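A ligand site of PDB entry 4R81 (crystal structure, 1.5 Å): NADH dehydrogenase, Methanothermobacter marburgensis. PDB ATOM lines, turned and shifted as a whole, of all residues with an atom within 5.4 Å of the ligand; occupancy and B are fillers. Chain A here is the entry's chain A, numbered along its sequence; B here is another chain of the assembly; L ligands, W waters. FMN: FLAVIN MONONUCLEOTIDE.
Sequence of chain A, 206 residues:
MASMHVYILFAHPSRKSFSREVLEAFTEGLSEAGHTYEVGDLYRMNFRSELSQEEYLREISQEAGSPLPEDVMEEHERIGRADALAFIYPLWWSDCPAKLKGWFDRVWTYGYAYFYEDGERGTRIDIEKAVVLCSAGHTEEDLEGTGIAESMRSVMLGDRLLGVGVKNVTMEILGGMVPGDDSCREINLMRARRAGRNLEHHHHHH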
ATOM      1  N   HIS A  12     -14.364  -4.771  36.903  1.00  0.00           N
ATOM      2  CA  HIS A  12     -15.133  -4.497  35.687  1.00  0.00           C
ATOM      3  C   HIS A  12     -15.800  -3.125  35.788  1.00  0.00           C
ATOM      4  O   HIS A  12     -16.386  -2.802  36.814  1.00  0.00           O
ATOM      5  CB  HIS A  12     -16.215  -5.565  35.451  1.00  0.00           C
ATOM      6  CG  HIS A  12     -16.701  -5.625  34.038  1.00  0.00           C
ATOM      7  ND1 HIS A  12     -17.406  -4.596  33.448  1.00  0.00           N
ATOM      8  CD2 HIS A  12     -16.573  -6.577  33.083  1.00  0.00           C
ATOM      9  CE1 HIS A  12     -17.691  -4.918  32.199  1.00  0.00           C
ATOM     10  NE2 HIS A  12     -17.199  -6.121  31.951  1.00  0.00           N
ATOM     11  N   SER A  17     -22.713  -6.684  33.451  1.00  0.00           N
ATOM     12  CA  SER A  17     -21.831  -7.415  32.555  1.00  0.00           C
ATOM     13  C   SER A  17     -21.921  -8.872  32.964  1.00  0.00           C
ATOM     14  O   SER A  17     -22.487  -9.195  33.998  1.00  0.00           O
ATOM     15  CB  SER A  17     -20.388  -6.947  32.707  1.00  0.00           C
ATOM     16  OG  SER A  17     -19.879  -7.272  33.985  1.00  0.00           O
ATOM     17  N   PHE A  18     -21.363  -9.747  32.148  1.00  0.00           N
ATOM     18  CA  PHE A  18     -21.359 -11.158  32.519  1.00  0.00           C
ATOM     19  C   PHE A  18     -20.537 -11.369  33.790  1.00  0.00           C
ATOM     20  O   PHE A  18     -20.904 -12.179  34.630  1.00  0.00           O
ATOM     21  CB  PHE A  18     -20.841 -12.020  31.367  1.00  0.00           C
ATOM     22  CG  PHE A  18     -20.820 -13.484  31.689  1.00  0.00           C
ATOM     23  CD1 PHE A  18     -21.998 -14.183  31.932  1.00  0.00           C
ATOM     24  CD2 PHE A  18     -19.611 -14.166  31.744  1.00  0.00           C
ATOM     25  CE1 PHE A  18     -21.974 -15.543  32.225  1.00  0.00           C
ATOM     26  CE2 PHE A  18     -19.588 -15.516  32.038  1.00  0.00           C
ATOM     27  CZ  PHE A  18     -20.758 -16.214  32.274  1.00  0.00           C
ATOM     28  N   SER A  19     -19.449 -10.612  33.942  1.00  0.00           N
ATOM     29  CA  SER A  19     -18.592 -10.758  35.110  1.00  0.00           C
ATOM     30  C   SER A  19     -19.380 -10.502  36.399  1.00  0.00           C
ATOM     31  O   SER A  19     -19.165 -11.160  37.427  1.00  0.00           O
ATOM     32  CB  SER A  19     -17.389  -9.817  35.022  1.00  0.00           C
ATOM     33  OG  SER A  19     -16.465 -10.294  34.041  1.00  0.00           O
ATOM     34  N   ARG A  20     -20.306  -9.557  36.355  1.00  0.00           N
ATOM     35  CA  ARG A  20     -21.170  -9.272  37.500  1.00  0.00           C
ATOM     36  C   ARG A  20     -22.064 -10.466  37.847  1.00  0.00           C
ATOM     37  O   ARG A  20     -22.263 -10.774  39.015  1.00  0.00           O
ATOM     38  CB  ARG A  20     -22.024  -8.024  37.230  1.00  0.00           C
ATOM     39  CG  ARG A  20     -22.896  -7.611  38.398  1.00  0.00           C
ATOM     40  CD  ARG A  20     -22.120  -6.766  39.385  1.00  0.00           C
ATOM     41  NE  ARG A  20     -21.531  -5.596  38.743  1.00  0.00           N
ATOM     42  CZ  ARG A  20     -20.745  -4.724  39.376  1.00  0.00           C
ATOM     43  NH1 ARG A  20     -20.469  -4.900  40.651  1.00  0.00           N
ATOM     44  NH2 ARG A  20     -20.234  -3.685  38.719  1.00  0.00           N
ATOM     45  N   PRO A  90     -12.957  -9.956  33.414  1.00  0.00           N
ATOM     46  CA  PRO A  90     -12.913 -10.366  32.011  1.00  0.00           C
ATOM     47  C   PRO A  90     -11.487 -10.402  31.473  1.00  0.00           C
ATOM     48  O   PRO A  90     -10.642  -9.578  31.860  1.00  0.00           O
ATOM     49  CB  PRO A  90     -13.696  -9.252  31.313  1.00  0.00           C
ATOM     50  CG  PRO A  90     -13.397  -8.037  32.138  1.00  0.00           C
ATOM     51  CD  PRO A  90     -13.316  -8.538  33.571  1.00  0.00           C
ATOM     52  N   LEU A  91     -11.227 -11.317  30.554  1.00  0.00           N
ATOM     53  CA  LEU A  91      -9.942 -11.429  29.889  1.00  0.00           C
ATOM     54  C   LEU A  91      -9.818 -10.315  28.873  1.00  0.00           C
ATOM     55  O   LEU A  91     -10.589 -10.276  27.911  1.00  0.00           O
ATOM     56  CB  LEU A  91      -9.830 -12.777  29.181  1.00  0.00           C
ATOM     57  CG  LEU A  91      -8.415 -13.093  28.698  1.00  0.00           C
ATOM     58  CD1 LEU A  91      -7.475 -13.031  29.899  1.00  0.00           C
ATOM     59  CD2 LEU A  91      -8.347 -14.455  28.014  1.00  0.00           C
ATOM     60  N   TRP A  92      -8.853  -9.424  29.070  1.00  0.00           N
ATOM     61  CA  TRP A  92      -8.586  -8.321  28.140  1.00  0.00           C
ATOM     62  C   TRP A  92      -7.131  -8.387  27.679  1.00  0.00           C
ATOM     63  O   TRP A  92      -6.214  -8.213  28.485  1.00  0.00           O
ATOM     64  CB  TRP A  92      -8.836  -6.957  28.798  1.00  0.00           C
ATOM     65  CG  TRP A  92     -10.271  -6.611  29.048  1.00  0.00           C
ATOM     66  CD1 TRP A  92     -11.371  -7.316  28.659  1.00  0.00           C
ATOM     67  CD2 TRP A  92     -10.760  -5.471  29.781  1.00  0.00           C
ATOM     68  NE1 TRP A  92     -12.520  -6.688  29.094  1.00  0.00           N
ATOM     69  CE2 TRP A  92     -12.170  -5.555  29.783  1.00  0.00           C
ATOM     70  CE3 TRP A  92     -10.144  -4.389  30.416  1.00  0.00           C
ATOM     71  CZ2 TRP A  92     -12.971  -4.596  30.407  1.00  0.00           C
ATOM     72  CZ3 TRP A  92     -10.938  -3.441  31.047  1.00  0.00           C
ATOM     73  CH2 TRP A  92     -12.341  -3.554  31.038  1.00  0.00           C
ATOM     74  N   TRP A  93      -6.930  -8.619  26.389  1.00  0.00           N
ATOM     75  CA  TRP A  93      -5.568  -8.745  25.842  1.00  0.00           C
ATOM     76  C   TRP A  93      -4.736  -9.741  26.644  1.00  0.00           C
ATOM     77  O   TRP A  93      -3.567  -9.530  26.965  1.00  0.00           O
ATOM     78  CB  TRP A  93      -4.910  -7.350  25.635  1.00  0.00           C
ATOM     79  CG  TRP A  93      -5.798  -6.570  24.707  1.00  0.00           C
ATOM     80  CD1 TRP A  93      -6.657  -5.563  25.040  1.00  0.00           C
ATOM     81  CD2 TRP A  93      -5.987  -6.810  23.304  1.00  0.00           C
ATOM     82  NE1 TRP A  93      -7.354  -5.148  23.912  1.00  0.00           N
ATOM     83  CE2 TRP A  93      -6.956  -5.900  22.838  1.00  0.00           C
ATOM     84  CE3 TRP A  93      -5.408  -7.702  22.388  1.00  0.00           C
ATOM     85  CZ2 TRP A  93      -7.370  -5.850  21.508  1.00  0.00           C
ATOM     86  CZ3 TRP A  93      -5.815  -7.653  21.066  1.00  0.00           C
ATOM     87  CH2 TRP A  93      -6.772  -6.727  20.631  1.00  0.00           C
ATOM     88  N   SER A  94      -5.400 -10.856  26.945  1.00  0.00           N
ATOM     89  CA  SER A  94      -4.773 -12.038  27.531  1.00  0.00           C
ATOM     90  C   SER A  94      -4.223 -11.846  28.945  1.00  0.00           C
ATOM     91  O   SER A  94      -3.387 -12.632  29.382  1.00  0.00           O
ATOM     92  CB  SER A  94      -3.717 -12.598  26.584  1.00  0.00           C
ATOM     93  OG  SER A  94      -4.322 -12.998  25.368  1.00  0.00           O
ATOM     94  N   SER A 135     -13.594 -14.578  32.693  1.00  0.00           N
ATOM     95  CA  SER A 135     -14.510 -14.689  31.559  1.00  0.00           C
ATOM     96  C   SER A 135     -13.779 -14.311  30.278  1.00  0.00           C
ATOM     97  O   SER A 135     -13.062 -13.312  30.252  1.00  0.00           O
ATOM     98  CB  SER A 135     -15.714 -13.768  31.758  1.00  0.00           C
ATOM     99  OG  SER A 135     -16.515 -13.713  30.596  1.00  0.00           O
ATOM    100  N   ALA A 136     -13.935 -15.101  29.220  1.00  0.00           N
ATOM    101  CA  ALA A 136     -13.207 -14.839  27.981  1.00  0.00           C
ATOM    102  C   ALA A 136     -14.096 -14.970  26.767  1.00  0.00           C
ATOM    103  O   ALA A 136     -15.031 -15.776  26.769  1.00  0.00           O
ATOM    104  CB  ALA A 136     -12.014 -15.780  27.857  1.00  0.00           C
ATOM    105  N   GLY A 137     -13.814 -14.185  25.732  1.00  0.00           N
ATOM    106  CA  GLY A 137     -14.495 -14.327  24.466  1.00  0.00           C
ATOM    107  C   GLY A 137     -14.158 -15.647  23.792  1.00  0.00           C
ATOM    108  O   GLY A 137     -15.032 -16.368  23.309  1.00  0.00           O
ATOM    109  N   HIS A 138     -12.858 -15.961  23.744  1.00  0.00           N
ATOM    110  CA  HIS A 138     -12.424 -17.247  23.203  1.00  0.00           C
ATOM    111  C   HIS A 138     -12.880 -18.388  24.093  1.00  0.00           C
ATOM    112  O   HIS A 138     -13.081 -18.216  25.296  1.00  0.00           O
ATOM    113  CB  HIS A 138     -10.912 -17.284  23.056  1.00  0.00           C
ATOM    114  CG  HIS A 138     -10.408 -16.518  21.876  1.00  0.00           C
ATOM    115  ND1 HIS A 138     -10.745 -16.855  20.579  1.00  0.00           N
ATOM    116  CD2 HIS A 138      -9.623 -15.420  21.789  1.00  0.00           C
ATOM    117  CE1 HIS A 138     -10.180 -16.003  19.744  1.00  0.00           C
ATOM    118  NE2 HIS A 138      -9.490 -15.121  20.450  1.00  0.00           N
ATOM    119  N   LEU A 143      -8.072 -21.224  23.760  1.00  0.00           N
ATOM    120  CA  LEU A 143      -6.994 -20.656  24.580  1.00  0.00           C
ATOM    121  C   LEU A 143      -5.966 -21.713  25.016  1.00  0.00           C
ATOM    122  O   LEU A 143      -4.773 -21.418  25.085  1.00  0.00           O
ATOM    123  CB  LEU A 143      -7.552 -19.937  25.817  1.00  0.00           C
ATOM    124  CG  LEU A 143      -8.393 -18.681  25.563  1.00  0.00           C
ATOM    125  CD1 LEU A 143      -8.957 -18.185  26.885  1.00  0.00           C
ATOM    126  CD2 LEU A 143      -7.590 -17.575  24.884  1.00  0.00           C
ATOM    127  N   MET A 177     -17.725 -16.276  25.628  1.00  0.00           N
ATOM    128  CA  MET A 177     -18.570 -15.103  25.849  1.00  0.00           C
ATOM    129  C   MET A 177     -18.289 -14.017  24.825  1.00  0.00           C
ATOM    130  O   MET A 177     -17.729 -12.962  25.131  1.00  0.00           O
ATOM    131  CB  MET A 177     -18.375 -14.572  27.269  1.00  0.00           C
ATOM    132  CG  MET A 177     -18.440 -15.645  28.359  1.00  0.00           C
ATOM    133  SD  MET A 177     -19.877 -16.721  28.234  1.00  0.00           S
ATOM    134  CE  MET A 177     -21.218 -15.566  28.555  1.00  0.00           C
ATOM    135  N   PRO A 179     -19.738 -11.179  22.102  1.00  0.00           N
ATOM    136  CA  PRO A 179     -20.898 -10.286  22.057  1.00  0.00           C
ATOM    137  C   PRO A 179     -22.054 -10.855  21.239  1.00  0.00           C
ATOM    138  O   PRO A 179     -21.857 -11.288  20.101  1.00  0.00           O
ATOM    139  CB  PRO A 179     -20.350  -9.032  21.381  1.00  0.00           C
ATOM    140  CG  PRO A 179     -18.901  -9.026  21.750  1.00  0.00           C
ATOM    141  CD  PRO A 179     -18.484 -10.469  21.780  1.00  0.00           C
ATOM    142  N   LEU B  51     -10.254   1.444  31.155  1.00  0.00           N
ATOM    143  CA  LEU B  51     -11.367   1.425  30.220  1.00  0.00           C
ATOM    144  C   LEU B  51     -12.625   1.773  31.011  1.00  0.00           C
ATOM    145  O   LEU B  51     -12.913   1.151  32.031  1.00  0.00           O
ATOM    146  CB  LEU B  51     -11.524   0.032  29.609  1.00  0.00           C
ATOM    147  CG  LEU B  51     -12.495  -0.127  28.451  1.00  0.00           C
ATOM    148  CD1 LEU B  51     -11.896   0.525  27.227  1.00  0.00           C
ATOM    149  CD2 LEU B  51     -12.767  -1.608  28.186  1.00  0.00           C
ATOM    150  N   TYR B  56     -16.288   0.584  27.304  1.00  0.00           N
ATOM    151  CA  TYR B  56     -16.601  -0.846  27.337  1.00  0.00           C
ATOM    152  C   TYR B  56     -17.850  -1.152  26.512  1.00  0.00           C
ATOM    153  O   TYR B  56     -17.851  -2.084  25.702  1.00  0.00           O
ATOM    154  CB  TYR B  56     -16.768  -1.340  28.776  1.00  0.00           C
ATOM    155  CG  TYR B  56     -17.490  -2.671  28.872  1.00  0.00           C
ATOM    156  CD1 TYR B  56     -16.815  -3.866  28.652  1.00  0.00           C
ATOM    157  CD2 TYR B  56     -18.842  -2.733  29.174  1.00  0.00           C
ATOM    158  CE1 TYR B  56     -17.472  -5.083  28.732  1.00  0.00           C
ATOM    159  CE2 TYR B  56     -19.514  -3.931  29.256  1.00  0.00           C
ATOM    160  CZ  TYR B  56     -18.832  -5.105  29.031  1.00  0.00           C
ATOM    161  OH  TYR B  56     -19.504  -6.304  29.127  1.00  0.00           O
ATOM    162  N   GLU B  59     -17.027  -0.849  22.904  1.00  0.00           N
ATOM    163  CA  GLU B  59     -16.263  -1.987  22.411  1.00  0.00           C
ATOM    164  C   GLU B  59     -17.154  -3.217  22.188  1.00  0.00           C
ATOM    165  O   GLU B  59     -17.057  -3.888  21.162  1.00  0.00           O
ATOM    166  CB  GLU B  59     -15.100  -2.313  23.354  1.00  0.00           C
ATOM    167  CG  GLU B  59     -14.045  -1.234  23.360  1.00  0.00           C
ATOM    168  CD  GLU B  59     -13.555  -0.875  21.968  1.00  0.00           C
ATOM    169  OE1 GLU B  59     -12.998  -1.768  21.287  1.00  0.00           O
ATOM    170  OE2 GLU B  59     -13.747   0.289  21.545  1.00  0.00           O
ATOM    171  N   ILE B  60     -18.027  -3.484  23.152  1.00  0.00           N
ATOM    172  CA  ILE B  60     -18.922  -4.634  23.090  1.00  0.00           C
ATOM    173  C   ILE B  60     -19.885  -4.519  21.918  1.00  0.00           C
ATOM    174  O   ILE B  60     -20.268  -5.520  21.302  1.00  0.00           O
ATOM    175  CB  ILE B  60     -19.712  -4.786  24.411  1.00  0.00           C
ATOM    176  CG1 ILE B  60     -18.768  -5.219  25.546  1.00  0.00           C
ATOM    177  CG2 ILE B  60     -20.864  -5.765  24.261  1.00  0.00           C
ATOM    178  CD1 ILE B  60     -17.974  -6.473  25.240  1.00  0.00           C
ATOM    179  N   ASP B 105      -5.756  -1.933  26.569  1.00  0.00           N
ATOM    180  CA  ASP B 105      -7.195  -2.047  26.793  1.00  0.00           C
ATOM    181  C   ASP B 105      -7.969  -0.950  26.072  1.00  0.00           C
ATOM    182  O   ASP B 105      -9.029  -1.208  25.502  1.00  0.00           O
ATOM    183  CB  ASP B 105      -7.536  -1.945  28.285  1.00  0.00           C
ATOM    184  CG  ASP B 105      -6.974  -3.077  29.109  1.00  0.00           C
ATOM    185  OD1 ASP B 105      -6.539  -4.108  28.544  1.00  0.00           O
ATOM    186  OD2 ASP B 105      -6.966  -2.928  30.352  1.00  0.00           O
ATOM    187  N   TYR B 114      -8.744  -4.730  15.681  1.00  0.00           N
ATOM    188  CA  TYR B 114      -9.399  -5.979  15.314  1.00  0.00           C
ATOM    189  C   TYR B 114     -10.847  -5.699  14.926  1.00  0.00           C
ATOM    190  O   TYR B 114     -11.495  -4.822  15.499  1.00  0.00           O
ATOM    191  CB  TYR B 114      -9.342  -6.969  16.481  1.00  0.00           C
ATOM    192  CG  TYR B 114     -10.236  -6.619  17.661  1.00  0.00           C
ATOM    193  CD1 TYR B 114      -9.872  -5.615  18.562  1.00  0.00           C
ATOM    194  CD2 TYR B 114     -11.434  -7.294  17.870  1.00  0.00           C
ATOM    195  CE1 TYR B 114     -10.682  -5.301  19.636  1.00  0.00           C
ATOM    196  CE2 TYR B 114     -12.243  -6.989  18.943  1.00  0.00           C
ATOM    197  CZ  TYR B 114     -11.870  -5.992  19.822  1.00  0.00           C
ATOM    198  OH  TYR B 114     -12.686  -5.696  20.886  1.00  0.00           O
ATOM    199  N   ASP B 159      -0.331 -12.227  21.113  1.00  0.00           N
ATOM    200  CA  ASP B 159      -1.689 -11.705  21.184  1.00  0.00           C
ATOM    201  C   ASP B 159      -1.777 -10.195  20.899  1.00  0.00           C
ATOM    202  O   ASP B 159      -2.633  -9.758  20.128  1.00  0.00           O
ATOM    203  CB  ASP B 159      -2.278 -12.003  22.563  1.00  0.00           C
ATOM    204  CG  ASP B 159      -3.770 -11.803  22.618  1.00  0.00           C
ATOM    205  OD1 ASP B 159      -4.465 -12.281  21.686  1.00  0.00           O
ATOM    206  OD2 ASP B 159      -4.261 -11.190  23.596  1.00  0.00           O
HETATM  207  N1  FMN L   1     -11.436 -12.331  24.922  1.00  0.00           N
HETATM  208  C2  FMN L   1     -10.414 -13.252  24.790  1.00  0.00           C
HETATM  209  O2  FMN L   1     -10.684 -14.444  24.706  1.00  0.00           O
HETATM  210  N3  FMN L   1      -9.101 -12.853  24.766  1.00  0.00           N
HETATM  211  C4  FMN L   1      -8.783 -11.511  24.866  1.00  0.00           C
HETATM  212  O4  FMN L   1      -7.598 -11.176  24.854  1.00  0.00           O
HETATM  213  C4A FMN L   1      -9.798 -10.570  24.994  1.00  0.00           C
HETATM  214  N5  FMN L   1      -9.514  -9.217  25.085  1.00  0.00           N
HETATM  215  C5A FMN L   1     -10.531  -8.297  25.225  1.00  0.00           C
HETATM  216  C6  FMN L   1     -10.227  -6.937  25.340  1.00  0.00           C
HETATM  217  C7  FMN L   1     -11.250  -6.006  25.474  1.00  0.00           C
HETATM  218  C7M FMN L   1     -10.927  -4.549  25.610  1.00  0.00           C
HETATM  219  C8  FMN L   1     -12.584  -6.426  25.500  1.00  0.00           C
HETATM  220  C8M FMN L   1     -13.692  -5.426  25.637  1.00  0.00           C
HETATM  221  C9  FMN L   1     -12.873  -7.785  25.386  1.00  0.00           C
HETATM  222  C9A FMN L   1     -11.850  -8.726  25.251  1.00  0.00           C
HETATM  223  N10 FMN L   1     -12.140 -10.076  25.138  1.00  0.00           N
HETATM  224  C10 FMN L   1     -11.118 -10.989  25.021  1.00  0.00           C
HETATM  225  C1' FMN L   1     -13.546 -10.571  25.193  1.00  0.00           C
HETATM  226  C2' FMN L   1     -13.937 -10.509  26.683  1.00  0.00           C
HETATM  227  O2' FMN L   1     -13.209 -11.433  27.467  1.00  0.00           O
HETATM  228  C3' FMN L   1     -15.444 -10.647  26.857  1.00  0.00           C
HETATM  229  O3' FMN L   1     -16.008  -9.439  26.379  1.00  0.00           O
HETATM  230  C4' FMN L   1     -15.797 -10.834  28.324  1.00  0.00           C
HETATM  231  O4' FMN L   1     -15.354 -12.084  28.810  1.00  0.00           O
HETATM  232  C5' FMN L   1     -17.294 -10.728  28.559  1.00  0.00           C
HETATM  233  O5' FMN L   1     -17.480 -10.621  29.955  1.00  0.00           O
HETATM  234  P   FMN L   1     -18.045  -9.252  30.542  1.00  0.00           P
HETATM  235  O1P FMN L   1     -19.472  -9.090  30.053  1.00  0.00           O
HETATM  236  O2P FMN L   1     -18.033  -9.310  32.051  1.00  0.00           O
HETATM  237  O3P FMN L   1     -17.203  -8.106  30.022  1.00  0.00           O
HETATM  238  O   HOH W   1     -15.215  -7.523  28.274  1.00  0.00           O
HETATM  239  O   HOH W   2     -12.055  -3.869  22.672  1.00  0.00           O
HETATM  240  O   HOH W   3      -6.639 -14.270  24.522  1.00  0.00           O
HETATM  241  O   HOH W   4      -9.386  -3.141  23.541  1.00  0.00           O
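The backbone carbonyl oxygen of Ser 135 sits at hydrogen-bond distance from an oxygen (O4') of the ligand (3.0 Å).
An oxygen (O4') of the ligand sits at hydrogen-bond distance from the side-chain hydroxyl of Ser 135 (2.7 Å).
An oxygen (O2P) of the ligand sits at hydrogen-bond distance from the backbone NH of Ser 19, at 2.7 Å.
OG of Ser 19 is in hydrogen-bond range of O2P of the ligand, 2.7 Å away.
O3P of the ligand is in hydrogen-bond range of NE2 of His 12, 2.8 Å away.
The backbone NH (N) of His 138 sits at hydrogen-bond distance from an oxygen (O2) of the ligand, 2.8 Å away.
N of Phe 18 is in hydrogen-bond range of O1P of the ligand, 2.9 Å away.
An oxygen (O2') of the ligand is in hydrogen-bond range of the backbone carbonyl oxygen (O) of Leu 91 (2.9 Å).
An oxygen (O1P) of the ligand lies within hydrogen-bond range of the side-chain hydroxyl of Tyr 56 of chain B (2.9 Å).
N of Trp 93 is in hydrogen-bond range of N5 of the ligand (3.0 Å).
N of Ser 94 lies within hydrogen-bond range of O4 of the ligand (3.1 Å).
A nitrogen (N1) of the ligand sits at hydrogen-bond distance from the backbone NH (N) of Gly 137.
The backbone NH (N) of Ala 136 lies within hydrogen-bond range of an oxygen (O4') of the ligand, at 3.4 Å.
An oxygen (O2P) of the ligand sits at hydrogen-bond distance from the side-chain hydroxyl (OG) of Ser 17 (3.4 Å).
The backbone carbonyl oxygen (O) of Ser 135 lies within hydrogen-bond range of the backbone NH (N) of Leu 91, at 2.7 Å.
The backbone NH of Ser 19 lies close to the side-chain hydroxyl of Ser 17, at 3.4 Å.
The side-chain hydroxyl (OG) of Ser 94 lies within hydrogen-bond range of the side-chain carboxylate (OD2) of Asp 159 of chain B.
N of Met 177 sits at hydrogen-bond distance from O of Ala 136, 3.0 Å away.
The backbone NH (N) of Arg 20 lies within hydrogen-bond range of the side-chain hydroxyl (OG) of Ser 17, at 3.3 Å.
Pro 90 touches the ligand.
Trp 92 touches the ligand (CA to N5, 3.3 Å).
Met 177 touches the ligand.
CD1 of Ile 60 of chain B touches O3' of the ligand (3.7 Å).
Asp 105 of chain B touches the ligand (O to C7M, 3.8 Å).
OD2 of Asp 159 of chain B touches O4 of the ligand, 3.6 Å away.
Of the 24 residues printed, 18 come within 4 Å of the ligand.
Water W1 bridges an oxygen (O3P) of the ligand (2.7 Å) and the indole nitrogen (NE1) of Trp 92 (2.9 Å).
Water W3 bridges OG of Ser 94 (2.8 Å) and N3 of the ligand (2.9 Å).
Water W4 bridges the backbone carbonyl oxygen of Asp 105 of chain B and the indole nitrogen of Trp 93.
Water W2 bridges the side-chain hydroxyl (OH) of Tyr 114 of chain B (2.6 Å) and the side-chain carboxylate (OE1) of Glu 59 of chain B (2.7 Å).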
